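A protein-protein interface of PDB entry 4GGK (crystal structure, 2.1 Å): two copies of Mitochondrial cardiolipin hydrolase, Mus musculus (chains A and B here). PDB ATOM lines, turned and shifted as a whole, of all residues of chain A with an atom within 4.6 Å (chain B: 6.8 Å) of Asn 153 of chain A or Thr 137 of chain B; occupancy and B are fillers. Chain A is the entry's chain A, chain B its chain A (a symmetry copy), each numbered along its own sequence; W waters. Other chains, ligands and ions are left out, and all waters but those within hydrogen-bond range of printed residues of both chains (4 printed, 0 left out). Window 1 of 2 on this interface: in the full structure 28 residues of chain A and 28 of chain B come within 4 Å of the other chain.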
ATOM      1  N   VAL A  11     -24.518  -2.176 -27.856  1.00  0.00           N
ATOM      2  CA  VAL A  11     -24.967  -2.893 -26.677  1.00  0.00           C
ATOM      3  C   VAL A  11     -25.456  -4.276 -27.124  1.00  0.00           C
ATOM      4  O   VAL A  11     -26.106  -4.423 -28.167  1.00  0.00           O
ATOM      5  CB  VAL A  11     -26.077  -2.096 -25.940  1.00  0.00           C
ATOM      6  CG1 VAL A  11     -27.127  -1.712 -26.893  1.00  0.00           C
ATOM      7  CG2 VAL A  11     -26.668  -2.904 -24.771  1.00  0.00           C
ATOM      8  N   LEU A  12     -25.075  -5.272 -26.343  1.00  0.00           N
ATOM      9  CA  LEU A  12     -25.430  -6.658 -26.549  1.00  0.00           C
ATOM     10  C   LEU A  12     -26.376  -6.996 -25.422  1.00  0.00           C
ATOM     11  O   LEU A  12     -26.055  -6.740 -24.239  1.00  0.00           O
ATOM     12  CB  LEU A  12     -24.196  -7.550 -26.399  1.00  0.00           C
ATOM     13  CG  LEU A  12     -22.948  -7.293 -27.219  1.00  0.00           C
ATOM     14  CD1 LEU A  12     -21.916  -8.372 -27.031  1.00  0.00           C
ATOM     15  CD2 LEU A  12     -23.342  -7.217 -28.619  1.00  0.00           C
ATOM     16  N   PHE A  13     -27.533  -7.554 -25.747  1.00  0.00           N
ATOM     17  CA  PHE A  13     -28.452  -8.026 -24.718  1.00  0.00           C
ATOM     18  C   PHE A  13     -28.436  -9.536 -24.632  1.00  0.00           C
ATOM     19  O   PHE A  13     -28.343 -10.241 -25.663  1.00  0.00           O
ATOM     20  CB  PHE A  13     -29.880  -7.511 -24.968  1.00  0.00           C
ATOM     21  CG  PHE A  13     -30.023  -6.044 -24.748  1.00  0.00           C
ATOM     22  CD1 PHE A  13     -29.883  -5.511 -23.473  1.00  0.00           C
ATOM     23  CD2 PHE A  13     -30.293  -5.183 -25.809  1.00  0.00           C
ATOM     24  CE1 PHE A  13     -30.002  -4.141 -23.257  1.00  0.00           C
ATOM     25  CE2 PHE A  13     -30.430  -3.817 -25.610  1.00  0.00           C
ATOM     26  CZ  PHE A  13     -30.280  -3.286 -24.339  1.00  0.00           C
ATOM     27  N   GLY A 138     -20.445  -4.355 -18.571  1.00  0.00           N
ATOM     28  CA  GLY A 138     -21.812  -4.829 -18.440  1.00  0.00           C
ATOM     29  C   GLY A 138     -22.277  -5.234 -17.047  1.00  0.00           C
ATOM     30  O   GLY A 138     -21.564  -5.097 -16.031  1.00  0.00           O
ATOM     31  N   SER A 139     -23.505  -5.729 -17.018  1.00  0.00           N
ATOM     32  CA  SER A 139     -24.040  -6.372 -15.847  1.00  0.00           C
ATOM     33  C   SER A 139     -23.566  -7.836 -15.810  1.00  0.00           C
ATOM     34  O   SER A 139     -23.654  -8.493 -14.755  1.00  0.00           O
ATOM     35  CB  SER A 139     -25.570  -6.327 -15.901  1.00  0.00           C
ATOM     36  OG  SER A 139     -26.045  -7.050 -17.018  1.00  0.00           O
ATOM     37  N   LEU A 140     -23.091  -8.335 -16.963  1.00  0.00           N
ATOM     38  CA  LEU A 140     -22.824  -9.773 -17.183  1.00  0.00           C
ATOM     39  C   LEU A 140     -21.560 -10.350 -16.530  1.00  0.00           C
ATOM     40  O   LEU A 140     -20.439  -9.957 -16.872  1.00  0.00           O
ATOM     41  CB  LEU A 140     -22.713 -10.043 -18.691  1.00  0.00           C
ATOM     42  CG  LEU A 140     -22.418 -11.473 -19.165  1.00  0.00           C
ATOM     43  CD1 LEU A 140     -23.626 -12.433 -18.919  1.00  0.00           C
ATOM     44  CD2 LEU A 140     -22.009 -11.435 -20.628  1.00  0.00           C
ATOM     45  N   GLU A 152     -29.179  -9.645 -19.311  1.00  0.00           N
ATOM     46  CA  GLU A 152     -27.976  -8.869 -19.060  1.00  0.00           C
ATOM     47  C   GLU A 152     -27.724  -7.877 -20.203  1.00  0.00           C
ATOM     48  O   GLU A 152     -28.273  -8.010 -21.297  1.00  0.00           O
ATOM     49  CB  GLU A 152     -26.768  -9.803 -18.973  1.00  0.00           C
ATOM     50  CG  GLU A 152     -26.947 -11.049 -18.118  1.00  0.00           C
ATOM     51  CD  GLU A 152     -26.427 -10.884 -16.691  1.00  0.00           C
ATOM     52  OE1 GLU A 152     -26.163  -9.759 -16.243  1.00  0.00           O
ATOM     53  OE2 GLU A 152     -26.322 -11.895 -15.999  1.00  0.00           O
ATOM     54  N   ASN A 153     -26.908  -6.865 -19.930  1.00  0.00           N
ATOM     55  CA  ASN A 153     -26.446  -5.958 -20.956  1.00  0.00           C
ATOM     56  C   ASN A 153     -24.932  -5.948 -20.884  1.00  0.00           C
ATOM     57  O   ASN A 153     -24.335  -6.097 -19.786  1.00  0.00           O
ATOM     58  CB  ASN A 153     -27.000  -4.539 -20.786  1.00  0.00           C
ATOM     59  CG  ASN A 153     -26.572  -3.890 -19.467  1.00  0.00           C
ATOM     60  OD1 ASN A 153     -27.222  -4.080 -18.429  1.00  0.00           O
ATOM     61  ND2 ASN A 153     -25.488  -3.130 -19.505  1.00  0.00           N
ATOM     62  N   VAL A 154     -24.329  -5.797 -22.056  1.00  0.00           N
ATOM     63  CA  VAL A 154     -22.894  -5.501 -22.214  1.00  0.00           C
ATOM     64  C   VAL A 154     -22.740  -4.338 -23.227  1.00  0.00           C
ATOM     65  O   VAL A 154     -23.262  -4.380 -24.340  1.00  0.00           O
ATOM     66  CB  VAL A 154     -22.122  -6.770 -22.624  1.00  0.00           C
ATOM     67  CG1 VAL A 154     -20.665  -6.461 -23.074  1.00  0.00           C
ATOM     68  CG2 VAL A 154     -22.096  -7.781 -21.428  1.00  0.00           C
ATOM     69  N   LEU A 155     -22.061  -3.281 -22.812  1.00  0.00           N
ATOM     70  CA  LEU A 155     -21.773  -2.149 -23.699  1.00  0.00           C
ATOM     71  C   LEU A 155     -20.385  -2.329 -24.289  1.00  0.00           C
ATOM     72  O   LEU A 155     -19.483  -2.824 -23.616  1.00  0.00           O
ATOM     73  CB  LEU A 155     -21.785  -0.851 -22.924  1.00  0.00           C
ATOM     74  CG  LEU A 155     -23.086  -0.557 -22.192  1.00  0.00           C
ATOM     75  CD1 LEU A 155     -22.885   0.677 -21.339  1.00  0.00           C
ATOM     76  CD2 LEU A 155     -24.237  -0.377 -23.174  1.00  0.00           C
ATOM     77  N   HIS B 124     -31.010  -9.806 -14.303  1.00  0.00           N
ATOM     78  CA  HIS B 124     -29.727  -9.417 -13.722  1.00  0.00           C
ATOM     79  C   HIS B 124     -29.253  -7.981 -14.120  1.00  0.00           C
ATOM     80  O   HIS B 124     -28.216  -7.528 -13.654  1.00  0.00           O
ATOM     81  CB  HIS B 124     -28.650 -10.471 -14.047  1.00  0.00           C
ATOM     82  CG  HIS B 124     -27.417 -10.385 -13.176  1.00  0.00           C
ATOM     83  ND1 HIS B 124     -26.254  -9.751 -13.573  1.00  0.00           N
ATOM     84  CD2 HIS B 124     -27.170 -10.859 -11.927  1.00  0.00           C
ATOM     85  CE1 HIS B 124     -25.354  -9.818 -12.608  1.00  0.00           C
ATOM     86  NE2 HIS B 124     -25.873 -10.502 -11.603  1.00  0.00           N
ATOM     87  N   HIS B 125     -30.020  -7.274 -14.944  1.00  0.00           N
ATOM     88  CA  HIS B 125     -29.752  -5.858 -15.222  1.00  0.00           C
ATOM     89  C   HIS B 125     -29.640  -4.996 -13.957  1.00  0.00           C
ATOM     90  O   HIS B 125     -30.253  -5.306 -12.933  1.00  0.00           O
ATOM     91  CB  HIS B 125     -30.842  -5.238 -16.082  1.00  0.00           C
ATOM     92  CG  HIS B 125     -30.973  -5.802 -17.470  1.00  0.00           C
ATOM     93  ND1 HIS B 125     -29.991  -5.683 -18.425  1.00  0.00           N
ATOM     94  CD2 HIS B 125     -32.015  -6.412 -18.080  1.00  0.00           C
ATOM     95  CE1 HIS B 125     -30.405  -6.225 -19.551  1.00  0.00           C
ATOM     96  NE2 HIS B 125     -31.634  -6.674 -19.369  1.00  0.00           N
ATOM     97  N   LYS B 126     -28.875  -3.899 -14.055  1.00  0.00           N
ATOM     98  CA  LYS B 126     -28.859  -2.851 -13.053  1.00  0.00           C
ATOM     99  C   LYS B 126     -28.905  -1.468 -13.700  1.00  0.00           C
ATOM    100  O   LYS B 126     -27.917  -0.722 -13.671  1.00  0.00           O
ATOM    101  CB  LYS B 126     -27.642  -2.956 -12.116  1.00  0.00           C
ATOM    102  CG  LYS B 126     -27.328  -4.372 -11.542  1.00  0.00           C
ATOM    103  CD  LYS B 126     -26.298  -5.072 -12.396  1.00  0.00           C
ATOM    104  CE  LYS B 126     -25.636  -6.255 -11.678  1.00  0.00           C
ATOM    105  NZ  LYS B 126     -26.629  -7.209 -11.223  1.00  0.00           N
ATOM    106  N   PHE B 127     -30.052  -1.123 -14.294  1.00  0.00           N
ATOM    107  CA  PHE B 127     -30.158   0.138 -15.015  1.00  0.00           C
ATOM    108  C   PHE B 127     -31.444   0.877 -14.701  1.00  0.00           C
ATOM    109  O   PHE B 127     -32.393   0.313 -14.152  1.00  0.00           O
ATOM    110  CB  PHE B 127     -29.960  -0.035 -16.539  1.00  0.00           C
ATOM    111  CG  PHE B 127     -31.143  -0.668 -17.283  1.00  0.00           C
ATOM    112  CD1 PHE B 127     -32.296   0.063 -17.560  1.00  0.00           C
ATOM    113  CD2 PHE B 127     -31.042  -1.965 -17.775  1.00  0.00           C
ATOM    114  CE1 PHE B 127     -33.365  -0.514 -18.263  1.00  0.00           C
ATOM    115  CE2 PHE B 127     -32.088  -2.564 -18.466  1.00  0.00           C
ATOM    116  CZ  PHE B 127     -33.264  -1.837 -18.710  1.00  0.00           C
ATOM    117  N   ALA B 128     -31.420   2.165 -15.032  1.00  0.00           N
ATOM    118  CA  ALA B 128     -32.529   3.070 -14.860  1.00  0.00           C
ATOM    119  C   ALA B 128     -32.515   4.066 -16.030  1.00  0.00           C
ATOM    120  O   ALA B 128     -31.458   4.403 -16.535  1.00  0.00           O
ATOM    121  CB  ALA B 128     -32.414   3.784 -13.556  1.00  0.00           C
ATOM    122  N   LEU B 135     -29.596   7.494 -19.527  1.00  0.00           N
ATOM    123  CA  LEU B 135     -29.388   6.103 -19.099  1.00  0.00           C
ATOM    124  C   LEU B 135     -28.405   6.028 -17.945  1.00  0.00           C
ATOM    125  O   LEU B 135     -27.301   6.559 -18.031  1.00  0.00           O
ATOM    126  CB  LEU B 135     -28.865   5.231 -20.258  1.00  0.00           C
ATOM    127  CG  LEU B 135     -28.516   3.760 -19.902  1.00  0.00           C
ATOM    128  CD1 LEU B 135     -29.724   3.056 -19.391  1.00  0.00           C
ATOM    129  CD2 LEU B 135     -27.947   3.033 -21.125  1.00  0.00           C
ATOM    130  N   ILE B 136     -28.823   5.358 -16.869  1.00  0.00           N
ATOM    131  CA  ILE B 136     -27.990   5.091 -15.722  1.00  0.00           C
ATOM    132  C   ILE B 136     -27.798   3.576 -15.676  1.00  0.00           C
ATOM    133  O   ILE B 136     -28.756   2.839 -15.506  1.00  0.00           O
ATOM    134  CB  ILE B 136     -28.659   5.537 -14.434  1.00  0.00           C
ATOM    135  CG1 ILE B 136     -28.776   7.070 -14.368  1.00  0.00           C
ATOM    136  CG2 ILE B 136     -27.858   5.051 -13.257  1.00  0.00           C
ATOM    137  CD1 ILE B 136     -29.807   7.534 -13.367  1.00  0.00           C
ATOM    138  N   THR B 137     -26.589   3.088 -15.896  1.00  0.00           N
ATOM    139  CA  THR B 137     -26.418   1.624 -15.914  1.00  0.00           C
ATOM    140  C   THR B 137     -25.069   1.248 -15.371  1.00  0.00           C
ATOM    141  O   THR B 137     -24.082   1.935 -15.625  1.00  0.00           O
ATOM    142  CB  THR B 137     -26.618   1.036 -17.337  1.00  0.00           C
ATOM    143  OG1 THR B 137     -26.563  -0.399 -17.288  1.00  0.00           O
ATOM    144  CG2 THR B 137     -25.556   1.572 -18.320  1.00  0.00           C
ATOM    145  N   GLY B 138     -25.029   0.145 -14.631  1.00  0.00           N
ATOM    146  CA  GLY B 138     -23.817  -0.261 -13.939  1.00  0.00           C
ATOM    147  C   GLY B 138     -23.684  -1.733 -13.574  1.00  0.00           C
ATOM    148  O   GLY B 138     -24.524  -2.592 -13.915  1.00  0.00           O
ATOM    149  N   SER B 139     -22.592  -2.013 -12.878  1.00  0.00           N
ATOM    150  CA  SER B 139     -22.397  -3.293 -12.249  1.00  0.00           C
ATOM    151  C   SER B 139     -23.134  -3.312 -10.897  1.00  0.00           C
ATOM    152  O   SER B 139     -23.354  -4.395 -10.322  1.00  0.00           O
ATOM    153  CB  SER B 139     -20.901  -3.521 -12.022  1.00  0.00           C
ATOM    154  OG  SER B 139     -20.381  -2.548 -11.140  1.00  0.00           O
ATOM    155  N   LEU B 140     -23.486  -2.116 -10.397  1.00  0.00           N
ATOM    156  CA  LEU B 140     -23.972  -1.920  -9.013  1.00  0.00           C
ATOM    157  C   LEU B 140     -25.415  -2.354  -8.719  1.00  0.00           C
ATOM    158  O   LEU B 140     -26.367  -1.792  -9.272  1.00  0.00           O
ATOM    159  CB  LEU B 140     -23.868  -0.432  -8.645  1.00  0.00           C
ATOM    160  CG  LEU B 140     -24.336   0.018  -7.255  1.00  0.00           C
ATOM    161  CD1 LEU B 140     -23.389  -0.493  -6.123  1.00  0.00           C
ATOM    162  CD2 LEU B 140     -24.470   1.532  -7.245  1.00  0.00           C
ATOM    163  N   ASN B 153     -19.007   0.160 -10.936  1.00  0.00           N
ATOM    164  CA  ASN B 153     -19.107   1.296 -11.823  1.00  0.00           C
ATOM    165  C   ASN B 153     -20.582   1.507 -12.102  1.00  0.00           C
ATOM    166  O   ASN B 153     -21.378   0.532 -12.148  1.00  0.00           O
ATOM    167  CB  ASN B 153     -18.338   1.094 -13.134  1.00  0.00           C
ATOM    168  CG  ASN B 153     -18.860  -0.089 -13.952  1.00  0.00           C
ATOM    169  OD1 ASN B 153     -18.447  -1.238 -13.737  1.00  0.00           O
ATOM    170  ND2 ASN B 153     -19.762   0.185 -14.883  1.00  0.00           N
ATOM    171  N   VAL B 154     -20.934   2.776 -12.260  1.00  0.00           N
ATOM    172  CA  VAL B 154     -22.240   3.211 -12.787  1.00  0.00           C
ATOM    173  C   VAL B 154     -21.998   4.290 -13.873  1.00  0.00           C
ATOM    174  O   VAL B 154     -21.307   5.283 -13.652  1.00  0.00           O
ATOM    175  CB  VAL B 154     -23.151   3.695 -11.642  1.00  0.00           C
ATOM    176  CG1 VAL B 154     -24.425   4.422 -12.162  1.00  0.00           C
ATOM    177  CG2 VAL B 154     -23.570   2.477 -10.751  1.00  0.00           C
ATOM    178  N   LEU B 155     -22.530   4.059 -15.062  1.00  0.00           N
ATOM    179  CA  LEU B 155     -22.445   5.038 -16.151  1.00  0.00           C
ATOM    180  C   LEU B 155     -23.719   5.865 -16.168  1.00  0.00           C
ATOM    181  O   LEU B 155     -24.799   5.348 -15.893  1.00  0.00           O
ATOM    182  CB  LEU B 155     -22.328   4.337 -17.486  1.00  0.00           C
ATOM    183  CG  LEU B 155     -21.142   3.392 -17.608  1.00  0.00           C
ATOM    184  CD1 LEU B 155     -21.256   2.652 -18.923  1.00  0.00           C
ATOM    185  CD2 LEU B 155     -19.824   4.151 -17.506  1.00  0.00           C
ATOM    186  N   ILE B 156     -23.587   7.154 -16.450  1.00  0.00           N
ATOM    187  CA  ILE B 156     -24.760   8.047 -16.576  1.00  0.00           C
ATOM    188  C   ILE B 156     -24.604   8.728 -17.926  1.00  0.00           C
ATOM    189  O   ILE B 156     -23.692   9.534 -18.128  1.00  0.00           O
ATOM    190  CB  ILE B 156     -24.829   9.076 -15.453  1.00  0.00           C
ATOM    191  CG1 ILE B 156     -24.882   8.367 -14.092  1.00  0.00           C
ATOM    192  CG2 ILE B 156     -26.056  10.006 -15.636  1.00  0.00           C
ATOM    193  CD1 ILE B 156     -24.751   9.302 -12.897  1.00  0.00           C
ATOM    194  N   MET B 157     -25.473   8.355 -18.854  1.00  0.00           N
ATOM    195  CA  MET B 157     -25.317   8.709 -20.270  1.00  0.00           C
ATOM    196  C   MET B 157     -26.591   9.258 -20.858  1.00  0.00           C
ATOM    197  O   MET B 157     -27.636   8.589 -20.845  1.00  0.00           O
ATOM    198  CB  MET B 157     -24.955   7.475 -21.097  1.00  0.00           C
ATOM    199  CG  MET B 157     -23.538   7.012 -20.933  1.00  0.00           C
ATOM    200  SD  MET B 157     -23.300   5.500 -21.901  1.00  0.00           S
ATOM    201  CE  MET B 157     -24.316   4.375 -20.910  1.00  0.00           C
ATOM    202  N   PHE B 166     -32.126   0.473 -24.679  1.00  0.00           N
ATOM    203  CA  PHE B 166     -32.444   0.060 -23.296  1.00  0.00           C
ATOM    204  C   PHE B 166     -33.926   0.221 -22.997  1.00  0.00           C
ATOM    205  O   PHE B 166     -34.510  -0.621 -22.324  1.00  0.00           O
ATOM    206  CB  PHE B 166     -31.617   0.820 -22.259  1.00  0.00           C
ATOM    207  CG  PHE B 166     -30.305   0.147 -21.911  1.00  0.00           C
ATOM    208  CD1 PHE B 166     -29.201   0.280 -22.731  1.00  0.00           C
ATOM    209  CD2 PHE B 166     -30.186  -0.620 -20.752  1.00  0.00           C
ATOM    210  CE1 PHE B 166     -27.956  -0.343 -22.405  1.00  0.00           C
ATOM    211  CE2 PHE B 166     -28.956  -1.222 -20.404  1.00  0.00           C
ATOM    212  CZ  PHE B 166     -27.843  -1.086 -21.242  1.00  0.00           C
ATOM    213  N   GLU B 169     -35.676  -2.728 -24.540  1.00  0.00           N
ATOM    214  CA  GLU B 169     -35.463  -3.916 -23.707  1.00  0.00           C
ATOM    215  C   GLU B 169     -36.369  -3.851 -22.484  1.00  0.00           C
ATOM    216  O   GLU B 169     -37.042  -4.834 -22.150  1.00  0.00           O
ATOM    217  CB  GLU B 169     -33.990  -4.065 -23.317  1.00  0.00           C
ATOM    218  CG  GLU B 169     -33.688  -5.118 -22.231  1.00  0.00           C
ATOM    219  CD  GLU B 169     -33.595  -6.560 -22.742  1.00  0.00           C
ATOM    220  OE1 GLU B 169     -34.136  -6.882 -23.818  1.00  0.00           O
ATOM    221  OE2 GLU B 169     -32.940  -7.376 -22.039  1.00  0.00           O
HETATM  222  O   HOH W   1     -26.719  -2.754 -15.749  1.00  0.00           O
HETATM  223  O   HOH W   2     -23.804  -1.502 -17.807  1.00  0.00           O
HETATM  224  O   HOH W   3     -24.230 -12.339 -14.509  1.00  0.00           O
HETATM  225  O   HOH W   4     -19.153  -3.711 -15.342  1.00  0.00           O
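O of Ser 139 of chain A sits close to ND1 of His 124 of chain B (3.1 Å).
ND1 of His 124 of chain B lies within hydrogen-bond range of OE1 of Glu 152 of chain A, at 2.7 Å.
The side-chain amide oxygen of Asn 153 of chain A sits at hydrogen-bond distance from a ring nitrogen (ND1) of His 125 of chain B (3.2 Å).
OE1 of Glu 152 of chain A sits at hydrogen-bond distance from OG of Ser 139 of chain A, 2.8 Å away.
N of Leu 140 of chain A is in hydrogen-bond range of OE1 of Glu 152 of chain A, 3.5 Å away.
The side-chain amino group (NZ) of Lys 126 of chain B is in hydrogen-bond range of the backbone carbonyl oxygen (O) of His 124 of chain B.
The side-chain carboxylate of Glu 169 of chain B sits at hydrogen-bond distance from a ring nitrogen (NE2) of His 125 of chain B, at 3.1 Å.
N of Gly 138 of chain B is in hydrogen-bond range of O of Lys 126 of chain B, 3.2 Å away.
The backbone carbonyl oxygen (O) of Thr 137 of chain B lies within hydrogen-bond range of the backbone NH (N) of Leu 155 of chain B (2.7 Å).
Among the printed residues, pairs that only touch across the chains: Val 11 of chain A with Phe 166 of chain B (3.7 Å), Phe 13 of chain A with Glu 169 of chain B (3.9 Å), Ser 139 of chain A with Lys 126 of chain B (3.8 Å), Glu 152 of chain A with His 125 of chain B (3.2 Å), Asn 153 of chain A with Thr 137 of chain B (3.7 Å), Asn 153 of chain A with Phe 166 of chain B (3.6 Å), Leu 155 of chain A with Leu 155 of chain B (3.5 Å), Leu 155 of chain A with Met 157 of chain B (3.99 Å) and Leu 155 of chain A with Phe 166 of chain B (3.8 Å).
Of the printed residues of chain A, Thr 137 of chain B touches Asn 153 (3.7 Å).
Of the printed residues of chain A, Glu 169 of chain B touches Phe 13.
Printed residues of chain A within 4 Å of His 124 of chain B: Ser 139 (3.0 Å) and Glu 152 (2.7 Å).
Of the printed residues of chain B, Glu 152 of chain A touches His 124 (2.7 Å) and His 125 (3.2 Å).
Of the printed residues of chain B, Phe 13 of chain A touches Glu 169.
Printed residues of chain A within 4 Å of Lys 126 of chain B: Ser 139.
Ala 128 of chain B touches none of the printed residues of chain A.
The nearest residue of chain A that does not touch Thr 137 of chain B is Leu 155 of chain A (4.1 Å).
The nearest printed residue of chain A that does not touch Met 157 of chain B is Asn 153 of chain A (7.7 Å).
Of the 18 printed residues of chain B, 8 touch a printed residue of chain A.
Along chain B the printed residues that touch a printed residue of chain A span positions 124 to 169.
Of the 10 printed residues of chain A, 6 touch a printed residue of chain B.
Hydrophobic or aromatic side chains of chain A within 4 Å of the printed part of chain B: Val 11, Phe 13 and Leu 155.
Among the printed residues, 12 pairs touch across the chains.
Leu 155 of chain B touches its own counterpart, Leu 155 of chain A.
Positions printed for both chains: 138, 139, 140, 153, 154 and 155.
Of the 12 pairs that touch across the chains among the printed residues, 1 has its exchanged pair printed and touching as well.
Water W3 lies within hydrogen-bond range of the side-chain carboxylate (OE2) of Glu 152 of chain A and a ring nitrogen (ND1) of His 124 of chain B.
Water W1 lies within hydrogen-bond range of OG1 of Thr 137 of chain B (2.8 Å), O of Gly 138 of chain B (2.9 Å), N of Lys 126 of chain B (3.0 Å) and OD1 of Asn 153 of chain A (3.0 Å).
Water W4 lies within hydrogen-bond range of the backbone carbonyl oxygen of Gly 138 of chain A and the side-chain amide oxygen of Asn 153 of chain B.
Water W2 lies within hydrogen-bond range of the side-chain amide nitrogen of Asn 153 of chain A and the side-chain hydroxyl of Thr 137 of chain B.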
